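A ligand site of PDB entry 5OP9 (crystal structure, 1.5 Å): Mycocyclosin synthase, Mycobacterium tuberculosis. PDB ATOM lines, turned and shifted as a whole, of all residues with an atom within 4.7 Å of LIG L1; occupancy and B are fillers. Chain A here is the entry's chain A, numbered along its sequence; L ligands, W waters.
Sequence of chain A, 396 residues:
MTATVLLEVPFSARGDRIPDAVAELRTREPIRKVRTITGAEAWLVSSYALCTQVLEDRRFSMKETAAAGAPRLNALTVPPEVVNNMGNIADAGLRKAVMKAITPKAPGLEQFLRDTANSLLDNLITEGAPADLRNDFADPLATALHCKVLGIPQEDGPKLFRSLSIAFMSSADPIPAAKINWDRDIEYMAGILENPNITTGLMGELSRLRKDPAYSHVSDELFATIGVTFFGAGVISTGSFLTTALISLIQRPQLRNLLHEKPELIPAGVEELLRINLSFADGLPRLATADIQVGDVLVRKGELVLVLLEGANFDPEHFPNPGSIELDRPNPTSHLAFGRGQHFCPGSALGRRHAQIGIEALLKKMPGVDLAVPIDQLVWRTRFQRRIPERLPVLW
An iron atom (FE1) of LIG L1 is bound by the side-chain sulfur (SG) of Cys 345 (2.3 Å). O1 of LIG L1 is in salt-bridge range of NH2 of Arg 286, at 2.7 Å. O3 of LIG L1 is in hydrogen-bond range of ND1 of His 343 (2.9 Å).
Water W3 lies within hydrogen-bond range of O1 of LIG L1 (2.7 Å) and O of His 343 (3.5 Å). Water W4 bridges an oxygen (O3) of LIG L1 (2.8 Å) and the backbone carbonyl oxygen of Phe 344 (2.8 Å). Water W5 lies within hydrogen-bond range of O of Gln 342 (2.9 Å), O3 of LIG L1 (3.0 Å) and ND1 of His 343 (3.5 Å).
The backbone carbonyl oxygen (O) of Phe 338 sits at hydrogen-bond distance from the backbone NH (N) of Cys 345, at 2.9 Å. N of Gly 347 sits close to SG of Cys 345, 3.3 Å away. SD of Met 62 lies within hydrogen-bond range of ND1 of His 343 (3.6 Å). The backbone carbonyl oxygen (O) of Ala 233 sits at hydrogen-bond distance from the side-chain hydroxyl (OG) of Ser 237 (2.7 Å). The backbone carbonyl oxygen (O) of Gly 234 is in hydrogen-bond range of the side-chain hydroxyl (OG1) of Thr 238 (2.7 Å).
SD of Met 62 lies close to O4 of LIG L1 (3.4 Å). Merely in contact with LIG L1: Met 86, Ala 337, Ser 237, Gly 339, Phe 280, Gly 234, His 146, Phe 338, Pro 346, Leu 284, Phe 230, Thr 238, Phe 241, Ala 233, Gly 347 and Leu 309. Hydrophobic or aromatic side chains within 4 Å of LIG L1: Met 62, Met 86, His 146, Phe 230, Ala 233, Phe 241, Phe 280, Leu 284, Leu 309, Phe 338, His 343 and Pro 346. Within 4 Å of LIG L1: Met 62, Met 86, His 146, Phe 230, Ala 233, Gly 234, Ser 237, Thr 238, Phe 241, Phe 280, Leu 284, Arg 286, Leu 309, Ala 337, Phe 338, Gly 339, His 343, Cys 345, Pro 346 and Gly 347.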
ATOM      1  N   MET A  62     -14.068 -26.257 -34.855  1.00  0.00           N
ATOM      2  CA  MET A  62     -12.828 -25.742 -35.455  1.00  0.00           C
ATOM      3  C   MET A  62     -12.224 -26.759 -36.406  1.00  0.00           C
ATOM      4  O   MET A  62     -11.887 -26.432 -37.547  1.00  0.00           O
ATOM      5  CB  MET A  62     -11.801 -25.375 -34.370  1.00  0.00           C
ATOM      6  CG  MET A  62     -10.396 -25.036 -34.933  1.00  0.00           C
ATOM      7  SD  MET A  62      -9.193 -24.692 -33.638  1.00  0.00           S
ATOM      8  CE  MET A  62      -9.746 -23.103 -33.081  1.00  0.00           C
ATOM      9  N   MET A  86      -4.684 -28.536 -30.986  1.00  0.00           N
ATOM     10  CA  MET A  86      -4.890 -28.752 -29.558  1.00  0.00           C
ATOM     11  C   MET A  86      -5.549 -30.099 -29.285  1.00  0.00           C
ATOM     12  O   MET A  86      -5.234 -30.757 -28.284  1.00  0.00           O
ATOM     13  CB  MET A  86      -5.690 -27.604 -28.942  1.00  0.00           C
ATOM     14  CG  MET A  86      -4.871 -26.339 -28.692  1.00  0.00           C
ATOM     15  SD  MET A  86      -3.437 -26.466 -27.608  1.00  0.00           S
ATOM     16  CE  MET A  86      -3.986 -27.681 -26.393  1.00  0.00           C
ATOM     17  N   ILE A 102       4.106 -23.057 -20.605  1.00  0.00           N
ATOM     18  CA  ILE A 102       3.889 -21.734 -21.176  1.00  0.00           C
ATOM     19  C   ILE A 102       3.218 -20.778 -20.199  1.00  0.00           C
ATOM     20  O   ILE A 102       2.722 -19.726 -20.609  1.00  0.00           O
ATOM     21  CB  ILE A 102       3.145 -21.800 -22.521  1.00  0.00           C
ATOM     22  CG1 ILE A 102       1.723 -22.312 -22.338  1.00  0.00           C
ATOM     23  CG2 ILE A 102       3.909 -22.680 -23.506  1.00  0.00           C
ATOM     24  CD1 ILE A 102       0.873 -22.216 -23.579  1.00  0.00           C
ATOM     25  N   HIS A 146       9.389 -15.789 -26.422  1.00  0.00           N
ATOM     26  CA  HIS A 146       9.044 -17.132 -26.866  1.00  0.00           C
ATOM     27  C   HIS A 146      10.257 -18.021 -27.055  1.00  0.00           C
ATOM     28  O   HIS A 146      10.144 -19.237 -26.848  1.00  0.00           O
ATOM     29  CB  HIS A 146       8.111 -17.074 -28.076  1.00  0.00           C
ATOM     30  CG  HIS A 146       6.722 -16.681 -27.705  1.00  0.00           C
ATOM     31  ND1 HIS A 146       6.366 -15.373 -27.460  1.00  0.00           N
ATOM     32  CD2 HIS A 146       5.637 -17.430 -27.413  1.00  0.00           C
ATOM     33  CE1 HIS A 146       5.110 -15.334 -27.070  1.00  0.00           C
ATOM     34  NE2 HIS A 146       4.637 -16.557 -27.041  1.00  0.00           N
ATOM     35  N   PHE A 230       3.298 -23.149 -31.423  1.00  0.00           N
ATOM     36  CA  PHE A 230       3.266 -22.323 -30.216  1.00  0.00           C
ATOM     37  C   PHE A 230       4.190 -21.111 -30.353  1.00  0.00           C
ATOM     38  O   PHE A 230       3.826 -20.001 -29.949  1.00  0.00           O
ATOM     39  CB  PHE A 230       3.532 -23.161 -28.963  1.00  0.00           C
ATOM     40  CG  PHE A 230       2.289 -23.802 -28.431  1.00  0.00           C
ATOM     41  CD1 PHE A 230       1.662 -24.812 -29.135  1.00  0.00           C
ATOM     42  CD2 PHE A 230       1.692 -23.349 -27.258  1.00  0.00           C
ATOM     43  CE1 PHE A 230       0.486 -25.386 -28.678  1.00  0.00           C
ATOM     44  CE2 PHE A 230       0.519 -23.915 -26.791  1.00  0.00           C
ATOM     45  CZ  PHE A 230      -0.080 -24.939 -27.503  1.00  0.00           C
ATOM     46  N   ALA A 233       2.101 -18.817 -33.104  1.00  0.00           N
ATOM     47  CA  ALA A 233       0.898 -18.222 -32.546  1.00  0.00           C
ATOM     48  C   ALA A 233       1.235 -17.251 -31.422  1.00  0.00           C
ATOM     49  O   ALA A 233       0.675 -16.155 -31.341  1.00  0.00           O
ATOM     50  CB  ALA A 233      -0.066 -19.308 -32.066  1.00  0.00           C
ATOM     51  N   GLY A 234       2.167 -17.643 -30.545  1.00  0.00           N
ATOM     52  CA  GLY A 234       2.505 -16.796 -29.417  1.00  0.00           C
ATOM     53  C   GLY A 234       3.155 -15.495 -29.838  1.00  0.00           C
ATOM     54  O   GLY A 234       2.776 -14.418 -29.384  1.00  0.00           O
ATOM     55  N   SER A 237       0.749 -13.246 -31.857  1.00  0.00           N
ATOM     56  CA  SER A 237      -0.377 -12.739 -31.069  1.00  0.00           C
ATOM     57  C   SER A 237       0.081 -11.698 -30.061  1.00  0.00           C
ATOM     58  O   SER A 237      -0.567 -10.653 -29.918  1.00  0.00           O
ATOM     59  CB  SER A 237      -1.108 -13.879 -30.373  1.00  0.00           C
ATOM     60  OG  SER A 237      -1.641 -14.781 -31.307  1.00  0.00           O
ATOM     61  N   THR A 238       1.182 -11.971 -29.354  1.00  0.00           N
ATOM     62  CA  THR A 238       1.666 -11.027 -28.343  1.00  0.00           C
ATOM     63  C   THR A 238       2.292  -9.792 -28.975  1.00  0.00           C
ATOM     64  O   THR A 238       2.056  -8.671 -28.511  1.00  0.00           O
ATOM     65  CB  THR A 238       2.676 -11.687 -27.383  1.00  0.00           C
ATOM     66  OG1 THR A 238       3.790 -12.229 -28.102  1.00  0.00           O
ATOM     67  CG2 THR A 238       2.003 -12.769 -26.558  1.00  0.00           C
ATOM     68  N   PHE A 241      -0.739  -7.790 -30.434  1.00  0.00           N
ATOM     69  CA  PHE A 241      -1.560  -7.212 -29.387  1.00  0.00           C
ATOM     70  C   PHE A 241      -0.833  -6.054 -28.713  1.00  0.00           C
ATOM     71  O   PHE A 241      -1.405  -4.965 -28.538  1.00  0.00           O
ATOM     72  CB  PHE A 241      -1.996  -8.228 -28.331  1.00  0.00           C
ATOM     73  CG  PHE A 241      -2.594  -7.552 -27.138  1.00  0.00           C
ATOM     74  CD1 PHE A 241      -3.783  -6.849 -27.277  1.00  0.00           C
ATOM     75  CD2 PHE A 241      -1.941  -7.508 -25.912  1.00  0.00           C
ATOM     76  CE1 PHE A 241      -4.312  -6.141 -26.228  1.00  0.00           C
ATOM     77  CE2 PHE A 241      -2.492  -6.806 -24.859  1.00  0.00           C
ATOM     78  CZ  PHE A 241      -3.677  -6.123 -25.012  1.00  0.00           C
ATOM     79  N   LEU A 274      -7.045  -5.378 -23.802  1.00  0.00           N
ATOM     80  CA  LEU A 274      -7.455  -6.629 -24.426  1.00  0.00           C
ATOM     81  C   LEU A 274      -8.892  -6.540 -24.919  1.00  0.00           C
ATOM     82  O   LEU A 274      -9.197  -6.912 -26.061  1.00  0.00           O
ATOM     83  CB  LEU A 274      -7.316  -7.786 -23.428  1.00  0.00           C
ATOM     84  CG  LEU A 274      -5.878  -8.295 -23.239  1.00  0.00           C
ATOM     85  CD1 LEU A 274      -5.781  -9.113 -21.971  1.00  0.00           C
ATOM     86  CD2 LEU A 274      -5.405  -9.101 -24.435  1.00  0.00           C
ATOM     87  N   SER A 279      -6.848  -6.643 -32.803  1.00  0.00           N
ATOM     88  CA  SER A 279      -5.727  -7.362 -33.403  1.00  0.00           C
ATOM     89  C   SER A 279      -6.171  -8.496 -34.324  1.00  0.00           C
ATOM     90  O   SER A 279      -5.535  -8.727 -35.340  1.00  0.00           O
ATOM     91  CB  SER A 279      -4.732  -7.866 -32.338  1.00  0.00           C
ATOM     92  OG  SER A 279      -5.154  -9.022 -31.642  1.00  0.00           O
ATOM     93  N   PHE A 280      -7.241  -9.222 -33.980  1.00  0.00           N
ATOM     94  CA  PHE A 280      -7.699 -10.274 -34.886  1.00  0.00           C
ATOM     95  C   PHE A 280      -8.396  -9.668 -36.088  1.00  0.00           C
ATOM     96  O   PHE A 280      -9.416  -8.982 -35.954  1.00  0.00           O
ATOM     97  CB  PHE A 280      -8.590 -11.285 -34.164  1.00  0.00           C
ATOM     98  CG  PHE A 280      -7.829 -12.391 -33.493  1.00  0.00           C
ATOM     99  CD1 PHE A 280      -6.960 -12.113 -32.452  1.00  0.00           C
ATOM    100  CD2 PHE A 280      -7.948 -13.695 -33.924  1.00  0.00           C
ATOM    101  CE1 PHE A 280      -6.241 -13.134 -31.844  1.00  0.00           C
ATOM    102  CE2 PHE A 280      -7.238 -14.703 -33.323  1.00  0.00           C
ATOM    103  CZ  PHE A 280      -6.382 -14.433 -32.290  1.00  0.00           C
ATOM    104  N   LEU A 284     -13.441 -15.482 -35.873  1.00  0.00           N
ATOM    105  CA  LEU A 284     -12.951 -16.842 -35.647  1.00  0.00           C
ATOM    106  C   LEU A 284     -13.835 -17.817 -36.421  1.00  0.00           C
ATOM    107  O   LEU A 284     -15.059 -17.803 -36.246  1.00  0.00           O
ATOM    108  CB  LEU A 284     -12.990 -17.197 -34.157  1.00  0.00           C
ATOM    109  CG  LEU A 284     -12.224 -16.278 -33.215  1.00  0.00           C
ATOM    110  CD1 LEU A 284     -12.383 -16.779 -31.783  1.00  0.00           C
ATOM    111  CD2 LEU A 284     -10.754 -16.174 -33.586  1.00  0.00           C
ATOM    112  N   ARG A 286     -15.689 -21.326 -37.668  1.00  0.00           N
ATOM    113  CA  ARG A 286     -16.230 -22.591 -37.201  1.00  0.00           C
ATOM    114  C   ARG A 286     -17.126 -23.143 -38.305  1.00  0.00           C
ATOM    115  O   ARG A 286     -17.768 -22.380 -39.034  1.00  0.00           O
ATOM    116  CB  ARG A 286     -17.105 -22.410 -35.960  1.00  0.00           C
ATOM    117  CG  ARG A 286     -16.373 -21.902 -34.718  1.00  0.00           C
ATOM    118  CD  ARG A 286     -15.386 -22.904 -34.180  1.00  0.00           C
ATOM    119  NE  ARG A 286     -14.839 -22.543 -32.870  1.00  0.00           N
ATOM    120  CZ  ARG A 286     -13.717 -21.840 -32.662  1.00  0.00           C
ATOM    121  NH1 ARG A 286     -13.019 -21.367 -33.677  1.00  0.00           N
ATOM    122  NH2 ARG A 286     -13.301 -21.622 -31.418  1.00  0.00           N
ATOM    123  N   LEU A 309     -14.842 -10.974 -32.890  1.00  0.00           N
ATOM    124  CA  LEU A 309     -14.501 -10.705 -31.502  1.00  0.00           C
ATOM    125  C   LEU A 309     -14.852  -9.283 -31.078  1.00  0.00           C
ATOM    126  O   LEU A 309     -15.334  -9.071 -29.960  1.00  0.00           O
ATOM    127  CB  LEU A 309     -13.037 -11.022 -31.240  1.00  0.00           C
ATOM    128  CG  LEU A 309     -12.633 -12.487 -31.433  1.00  0.00           C
ATOM    129  CD1 LEU A 309     -11.156 -12.657 -31.124  1.00  0.00           C
ATOM    130  CD2 LEU A 309     -13.491 -13.444 -30.596  1.00  0.00           C
ATOM    131  N   LEU A 336     -13.933 -11.486 -24.916  1.00  0.00           N
ATOM    132  CA  LEU A 336     -13.585 -12.621 -25.763  1.00  0.00           C
ATOM    133  C   LEU A 336     -12.227 -12.465 -26.455  1.00  0.00           C
ATOM    134  O   LEU A 336     -11.971 -13.126 -27.466  1.00  0.00           O
ATOM    135  CB  LEU A 336     -14.674 -12.858 -26.798  1.00  0.00           C
ATOM    136  CG  LEU A 336     -16.102 -13.047 -26.261  1.00  0.00           C
ATOM    137  CD1 LEU A 336     -17.004 -13.567 -27.370  1.00  0.00           C
ATOM    138  CD2 LEU A 336     -16.156 -13.944 -25.057  1.00  0.00           C
ATOM    139  N   ALA A 337     -11.336 -11.629 -25.927  1.00  0.00           N
ATOM    140  CA  ALA A 337     -10.051 -11.430 -26.610  1.00  0.00           C
ATOM    141  C   ALA A 337      -9.242 -12.722 -26.734  1.00  0.00           C
ATOM    142  O   ALA A 337      -8.449 -12.857 -27.664  1.00  0.00           O
ATOM    143  CB  ALA A 337      -9.208 -10.369 -25.899  1.00  0.00           C
ATOM    144  N   PHE A 338      -9.411 -13.663 -25.791  1.00  0.00           N
ATOM    145  CA  PHE A 338      -8.748 -14.958 -25.816  1.00  0.00           C
ATOM    146  C   PHE A 338      -9.677 -16.082 -26.251  1.00  0.00           C
ATOM    147  O   PHE A 338      -9.362 -17.262 -26.060  1.00  0.00           O
ATOM    148  CB  PHE A 338      -8.182 -15.282 -24.427  1.00  0.00           C
ATOM    149  CG  PHE A 338      -7.068 -14.367 -23.984  1.00  0.00           C
ATOM    150  CD1 PHE A 338      -5.876 -14.311 -24.698  1.00  0.00           C
ATOM    151  CD2 PHE A 338      -7.203 -13.577 -22.844  1.00  0.00           C
ATOM    152  CE1 PHE A 338      -4.844 -13.469 -24.290  1.00  0.00           C
ATOM    153  CE2 PHE A 338      -6.170 -12.746 -22.427  1.00  0.00           C
ATOM    154  CZ  PHE A 338      -4.990 -12.687 -23.150  1.00  0.00           C
ATOM    155  N   GLY A 339     -10.816 -15.741 -26.849  1.00  0.00           N
ATOM    156  CA  GLY A 339     -11.795 -16.732 -27.185  1.00  0.00           C
ATOM    157  C   GLY A 339     -12.613 -17.172 -25.978  1.00  0.00           C
ATOM    158  O   GLY A 339     -12.715 -16.468 -24.960  1.00  0.00           O
ATOM    159  N   GLN A 342     -14.059 -24.498 -25.754  1.00  0.00           N
ATOM    160  CA  GLN A 342     -13.089 -25.565 -25.972  1.00  0.00           C
ATOM    161  C   GLN A 342     -11.731 -25.024 -26.427  1.00  0.00           C
ATOM    162  O   GLN A 342     -10.690 -25.589 -26.066  1.00  0.00           O
ATOM    163  CB  GLN A 342     -13.646 -26.533 -27.012  1.00  0.00           C
ATOM    164  CG  GLN A 342     -12.731 -27.688 -27.375  1.00  0.00           C
ATOM    165  CD  GLN A 342     -12.677 -28.726 -26.282  1.00  0.00           C
ATOM    166  OE1 GLN A 342     -13.465 -28.705 -25.337  1.00  0.00           O
ATOM    167  NE2 GLN A 342     -11.747 -29.662 -26.402  1.00  0.00           N
ATOM    168  N   HIS A 343     -11.705 -23.948 -27.221  1.00  0.00           N
ATOM    169  CA  HIS A 343     -10.467 -23.482 -27.838  1.00  0.00           C
ATOM    170  C   HIS A 343      -9.926 -22.204 -27.204  1.00  0.00           C
ATOM    171  O   HIS A 343      -9.117 -21.515 -27.821  1.00  0.00           O
ATOM    172  CB  HIS A 343     -10.660 -23.327 -29.341  1.00  0.00           C
ATOM    173  CG  HIS A 343     -10.973 -24.623 -30.010  1.00  0.00           C
ATOM    174  ND1 HIS A 343     -10.007 -25.575 -30.242  1.00  0.00           N
ATOM    175  CD2 HIS A 343     -12.134 -25.153 -30.434  1.00  0.00           C
ATOM    176  CE1 HIS A 343     -10.559 -26.633 -30.803  1.00  0.00           C
ATOM    177  NE2 HIS A 343     -11.854 -26.402 -30.934  1.00  0.00           N
ATOM    178  N   PHE A 344     -10.325 -21.907 -25.957  1.00  0.00           N
ATOM    179  CA  PHE A 344      -9.797 -20.758 -25.236  1.00  0.00           C
ATOM    180  C   PHE A 344      -8.272 -20.760 -25.272  1.00  0.00           C
ATOM    181  O   PHE A 344      -7.636 -21.805 -25.084  1.00  0.00           O
ATOM    182  CB  PHE A 344     -10.282 -20.824 -23.776  1.00  0.00           C
ATOM    183  CG  PHE A 344      -9.865 -19.643 -22.967  1.00  0.00           C
ATOM    184  CD1 PHE A 344     -10.604 -18.482 -22.997  1.00  0.00           C
ATOM    185  CD2 PHE A 344      -8.715 -19.686 -22.208  1.00  0.00           C
ATOM    186  CE1 PHE A 344     -10.204 -17.372 -22.267  1.00  0.00           C
ATOM    187  CE2 PHE A 344      -8.309 -18.597 -21.481  1.00  0.00           C
ATOM    188  CZ  PHE A 344      -9.048 -17.425 -21.520  1.00  0.00           C
ATOM    189  N   CYS A 345      -7.688 -19.587 -25.514  1.00  0.00           N
ATOM    190  CA  CYS A 345      -6.252 -19.463 -25.722  1.00  0.00           C
ATOM    191  C   CYS A 345      -5.458 -20.102 -24.574  1.00  0.00           C
ATOM    192  O   CYS A 345      -5.588 -19.670 -23.433  1.00  0.00           O
ATOM    193  CB  CYS A 345      -5.878 -17.983 -25.779  1.00  0.00           C
ATOM    194  SG  CYS A 345      -4.116 -17.739 -26.054  1.00  0.00           S
ATOM    195  N   PRO A 346      -4.592 -21.081 -24.862  1.00  0.00           N
ATOM    196  CA  PRO A 346      -3.742 -21.650 -23.798  1.00  0.00           C
ATOM    197  C   PRO A 346      -2.616 -20.737 -23.346  1.00  0.00           C
ATOM    198  O   PRO A 346      -1.997 -21.026 -22.313  1.00  0.00           O
ATOM    199  CB  PRO A 346      -3.189 -22.922 -24.455  1.00  0.00           C
ATOM    200  CG  PRO A 346      -3.110 -22.557 -25.911  1.00  0.00           C
ATOM    201  CD  PRO A 346      -4.332 -21.714 -26.168  1.00  0.00           C
ATOM    202  N   GLY A 347      -2.339 -19.664 -24.076  1.00  0.00           N
ATOM    203  CA  GLY A 347      -1.299 -18.727 -23.708  1.00  0.00           C
ATOM    204  C   GLY A 347      -1.787 -17.458 -23.032  1.00  0.00           C
ATOM    205  O   GLY A 347      -1.031 -16.481 -22.953  1.00  0.00           O
ATOM    206  N   LEU A 350       0.402 -15.836 -20.286  1.00  0.00           N
ATOM    207  CA  LEU A 350       1.647 -15.346 -20.839  1.00  0.00           C
ATOM    208  C   LEU A 350       1.428 -14.080 -21.663  1.00  0.00           C
ATOM    209  O   LEU A 350       2.249 -13.151 -21.634  1.00  0.00           O
ATOM    210  CB  LEU A 350       2.280 -16.452 -21.685  1.00  0.00           C
ATOM    211  CG  LEU A 350       3.701 -16.214 -22.193  1.00  0.00           C
ATOM    212  CD1 LEU A 350       4.698 -16.124 -21.037  1.00  0.00           C
ATOM    213  CD2 LEU A 350       4.085 -17.313 -23.144  1.00  0.00           C
ATOM    214  N   GLY A 351       0.332 -14.027 -22.421  1.00  0.00           N
ATOM    215  CA  GLY A 351       0.055 -12.844 -23.215  1.00  0.00           C
ATOM    216  C   GLY A 351      -0.235 -11.642 -22.340  1.00  0.00           C
ATOM    217  O   GLY A 351       0.239 -10.538 -22.611  1.00  0.00           O
HETATM  218  C1  LIG L   1      -6.036 -19.635 -29.423  1.00  0.00           C
HETATM  219  C2  LIG L   1      -5.825 -14.837 -28.847  1.00  0.00           C
HETATM  220  C3  LIG L   1      -1.371 -15.312 -26.983  1.00  0.00           C
HETATM  221  C4  LIG L   1      -1.290 -19.871 -28.548  1.00  0.00           C
HETATM  222  C5  LIG L   1      -6.414 -18.317 -29.337  1.00  0.00           C
HETATM  223  C6  LIG L   1      -7.739 -17.782 -29.595  1.00  0.00           C
HETATM  224  C7  LIG L   1      -7.671 -16.448 -29.470  1.00  0.00           C
HETATM  225  C8  LIG L   1      -6.322 -16.100 -29.096  1.00  0.00           C
HETATM  226  C9  LIG L   1      -8.824 -15.449 -29.668  1.00  0.00           C
HETATM  227  C10 LIG L   1      -8.981 -18.641 -29.955  1.00  0.00           C
HETATM  228  C11 LIG L   1      -9.026 -19.039 -31.408  1.00  0.00           C
HETATM  229  C12 LIG L   1     -10.312 -19.749 -31.750  1.00  0.00           C
HETATM  230  O1  LIG L   1     -11.094 -20.145 -30.842  1.00  0.00           O
HETATM  231  O2  LIG L   1     -10.557 -19.971 -32.965  1.00  0.00           O
HETATM  232  C13 LIG L   1      -4.601 -14.536 -28.291  1.00  0.00           C
HETATM  233  C14 LIG L   1      -4.157 -13.232 -27.841  1.00  0.00           C
HETATM  234  C15 LIG L   1      -2.914 -13.367 -27.348  1.00  0.00           C
HETATM  235  C16 LIG L   1      -2.541 -14.765 -27.444  1.00  0.00           C
HETATM  236  C17 LIG L   1      -4.998 -11.958 -28.000  1.00  0.00           C
HETATM  237  C18 LIG L   1      -1.980 -12.313 -26.738  1.00  0.00           C
HETATM  238  C19 LIG L   1      -2.435 -11.217 -26.123  1.00  0.00           C
HETATM  239  C20 LIG L   1      -0.966 -16.613 -27.195  1.00  0.00           C
HETATM  240  C21 LIG L   1       0.295 -17.194 -26.765  1.00  0.00           C
HETATM  241  C22 LIG L   1       0.314 -18.462 -27.207  1.00  0.00           C
HETATM  242  C23 LIG L   1      -0.933 -18.703 -27.915  1.00  0.00           C
HETATM  243  C24 LIG L   1       1.336 -16.384 -25.952  1.00  0.00           C
HETATM  244  C25 LIG L   1       1.390 -19.553 -27.058  1.00  0.00           C
HETATM  245  C26 LIG L   1       2.593 -19.403 -26.488  1.00  0.00           C
HETATM  246  C27 LIG L   1      -2.550 -20.201 -28.957  1.00  0.00           C
HETATM  247  C28 LIG L   1      -2.985 -21.478 -29.487  1.00  0.00           C
HETATM  248  C29 LIG L   1      -4.316 -21.433 -29.739  1.00  0.00           C
HETATM  249  C30 LIG L   1      -4.742 -20.094 -29.363  1.00  0.00           C
HETATM  250  C31 LIG L   1      -2.017 -22.665 -29.720  1.00  0.00           C
HETATM  251  C32 LIG L   1      -5.248 -22.533 -30.304  1.00  0.00           C
HETATM  252  C33 LIG L   1      -6.063 -23.141 -29.151  1.00  0.00           C
HETATM  253  C34 LIG L   1      -7.054 -24.202 -29.587  1.00  0.00           C
HETATM  254  O3  LIG L   1      -7.632 -24.899 -28.707  1.00  0.00           O
HETATM  255  O4  LIG L   1      -7.274 -24.398 -30.804  1.00  0.00           O
HETATM  256  N1  LIG L   1      -5.563 -17.259 -29.018  1.00  0.00           N
HETATM  257  N2  LIG L   1      -3.585 -15.443 -28.034  1.00  0.00           N
HETATM  258  N3  LIG L   1      -1.691 -17.555 -27.881  1.00  0.00           N
HETATM  259  N4  LIG L   1      -3.655 -19.381 -28.891  1.00  0.00           N
HETATM  260 FE1  LIG L   1      -3.689 -17.441 -28.304  1.00  0.00          FE
HETATM  261  C1  LG2 L   2      -4.975 -24.753 -33.142  1.00  0.00           C
HETATM  262  C2  LG2 L   2      -2.989 -23.782 -33.844  1.00  0.00           C
HETATM  263  C3  LG2 L   2      -1.801 -23.128 -33.584  1.00  0.00           C
HETATM  264  C4  LG2 L   2      -1.123 -22.517 -34.607  1.00  0.00           C
HETATM  265  C5  LG2 L   2      -1.606 -22.576 -35.899  1.00  0.00           C
HETATM  266  C6  LG2 L   2      -0.823 -21.932 -36.938  1.00  0.00           C
HETATM  267  C7  LG2 L   2       2.282 -21.345 -38.216  1.00  0.00           C
HETATM  268  C8  LG2 L   2       3.099 -21.073 -37.124  1.00  0.00           C
HETATM  269  C9  LG2 L   2       4.454 -20.996 -37.332  1.00  0.00           C
HETATM  270  C10 LG2 L   2       4.945 -21.194 -38.614  1.00  0.00           C
HETATM  271  C11 LG2 L   2       4.097 -21.454 -39.668  1.00  0.00           C
HETATM  272  C12 LG2 L   2       2.733 -21.547 -39.490  1.00  0.00           C
HETATM  273  C13 LG2 L   2      -0.110 -20.747 -38.672  1.00  0.00           C
HETATM  274  C14 LG2 L   2      -1.277 -21.099 -38.002  1.00  0.00           C
HETATM  275  C15 LG2 L   2      -2.683 -20.676 -38.312  1.00  0.00           C
HETATM  276  C16 LG2 L   2      -2.999 -21.459 -40.740  1.00  0.00           C
HETATM  277  C17 LG2 L   2      -3.998 -22.182 -41.375  1.00  0.00           C
HETATM  278  C18 LG2 L   2      -4.621 -22.031 -39.273  1.00  0.00           C
HETATM  279  C19 LG2 L   2      -2.790 -23.228 -36.191  1.00  0.00           C
HETATM  280  C20 LG2 L   2      -3.487 -23.835 -35.163  1.00  0.00           C
HETATM  281  N1  LG2 L   2       0.478 -22.091 -36.932  1.00  0.00           N
HETATM  282  N2  LG2 L   2       0.876 -21.419 -37.955  1.00  0.00           N
HETATM  283  N3  LG2 L   2      -3.387 -21.359 -39.388  1.00  0.00           N
HETATM  284  N4  LG2 L   2      -5.001 -22.548 -40.461  1.00  0.00           N
HETATM  285  O1  LG2 L   2      -3.655 -24.351 -32.848  1.00  0.00           O
HETATM  286  O   HOH W   1      -9.011 -19.708 -35.086  1.00  0.00           O
HETATM  287  O   HOH W   2      -3.057 -17.015 -30.463  1.00  0.00           O
HETATM  288  O   HOH W   3     -12.141 -19.852 -28.362  1.00  0.00           O
HETATM  289  O   HOH W   4      -7.182 -24.402 -26.015  1.00  0.00           O
HETATM  290  O   HOH W   5      -8.831 -27.306 -27.446  1.00  0.00           O
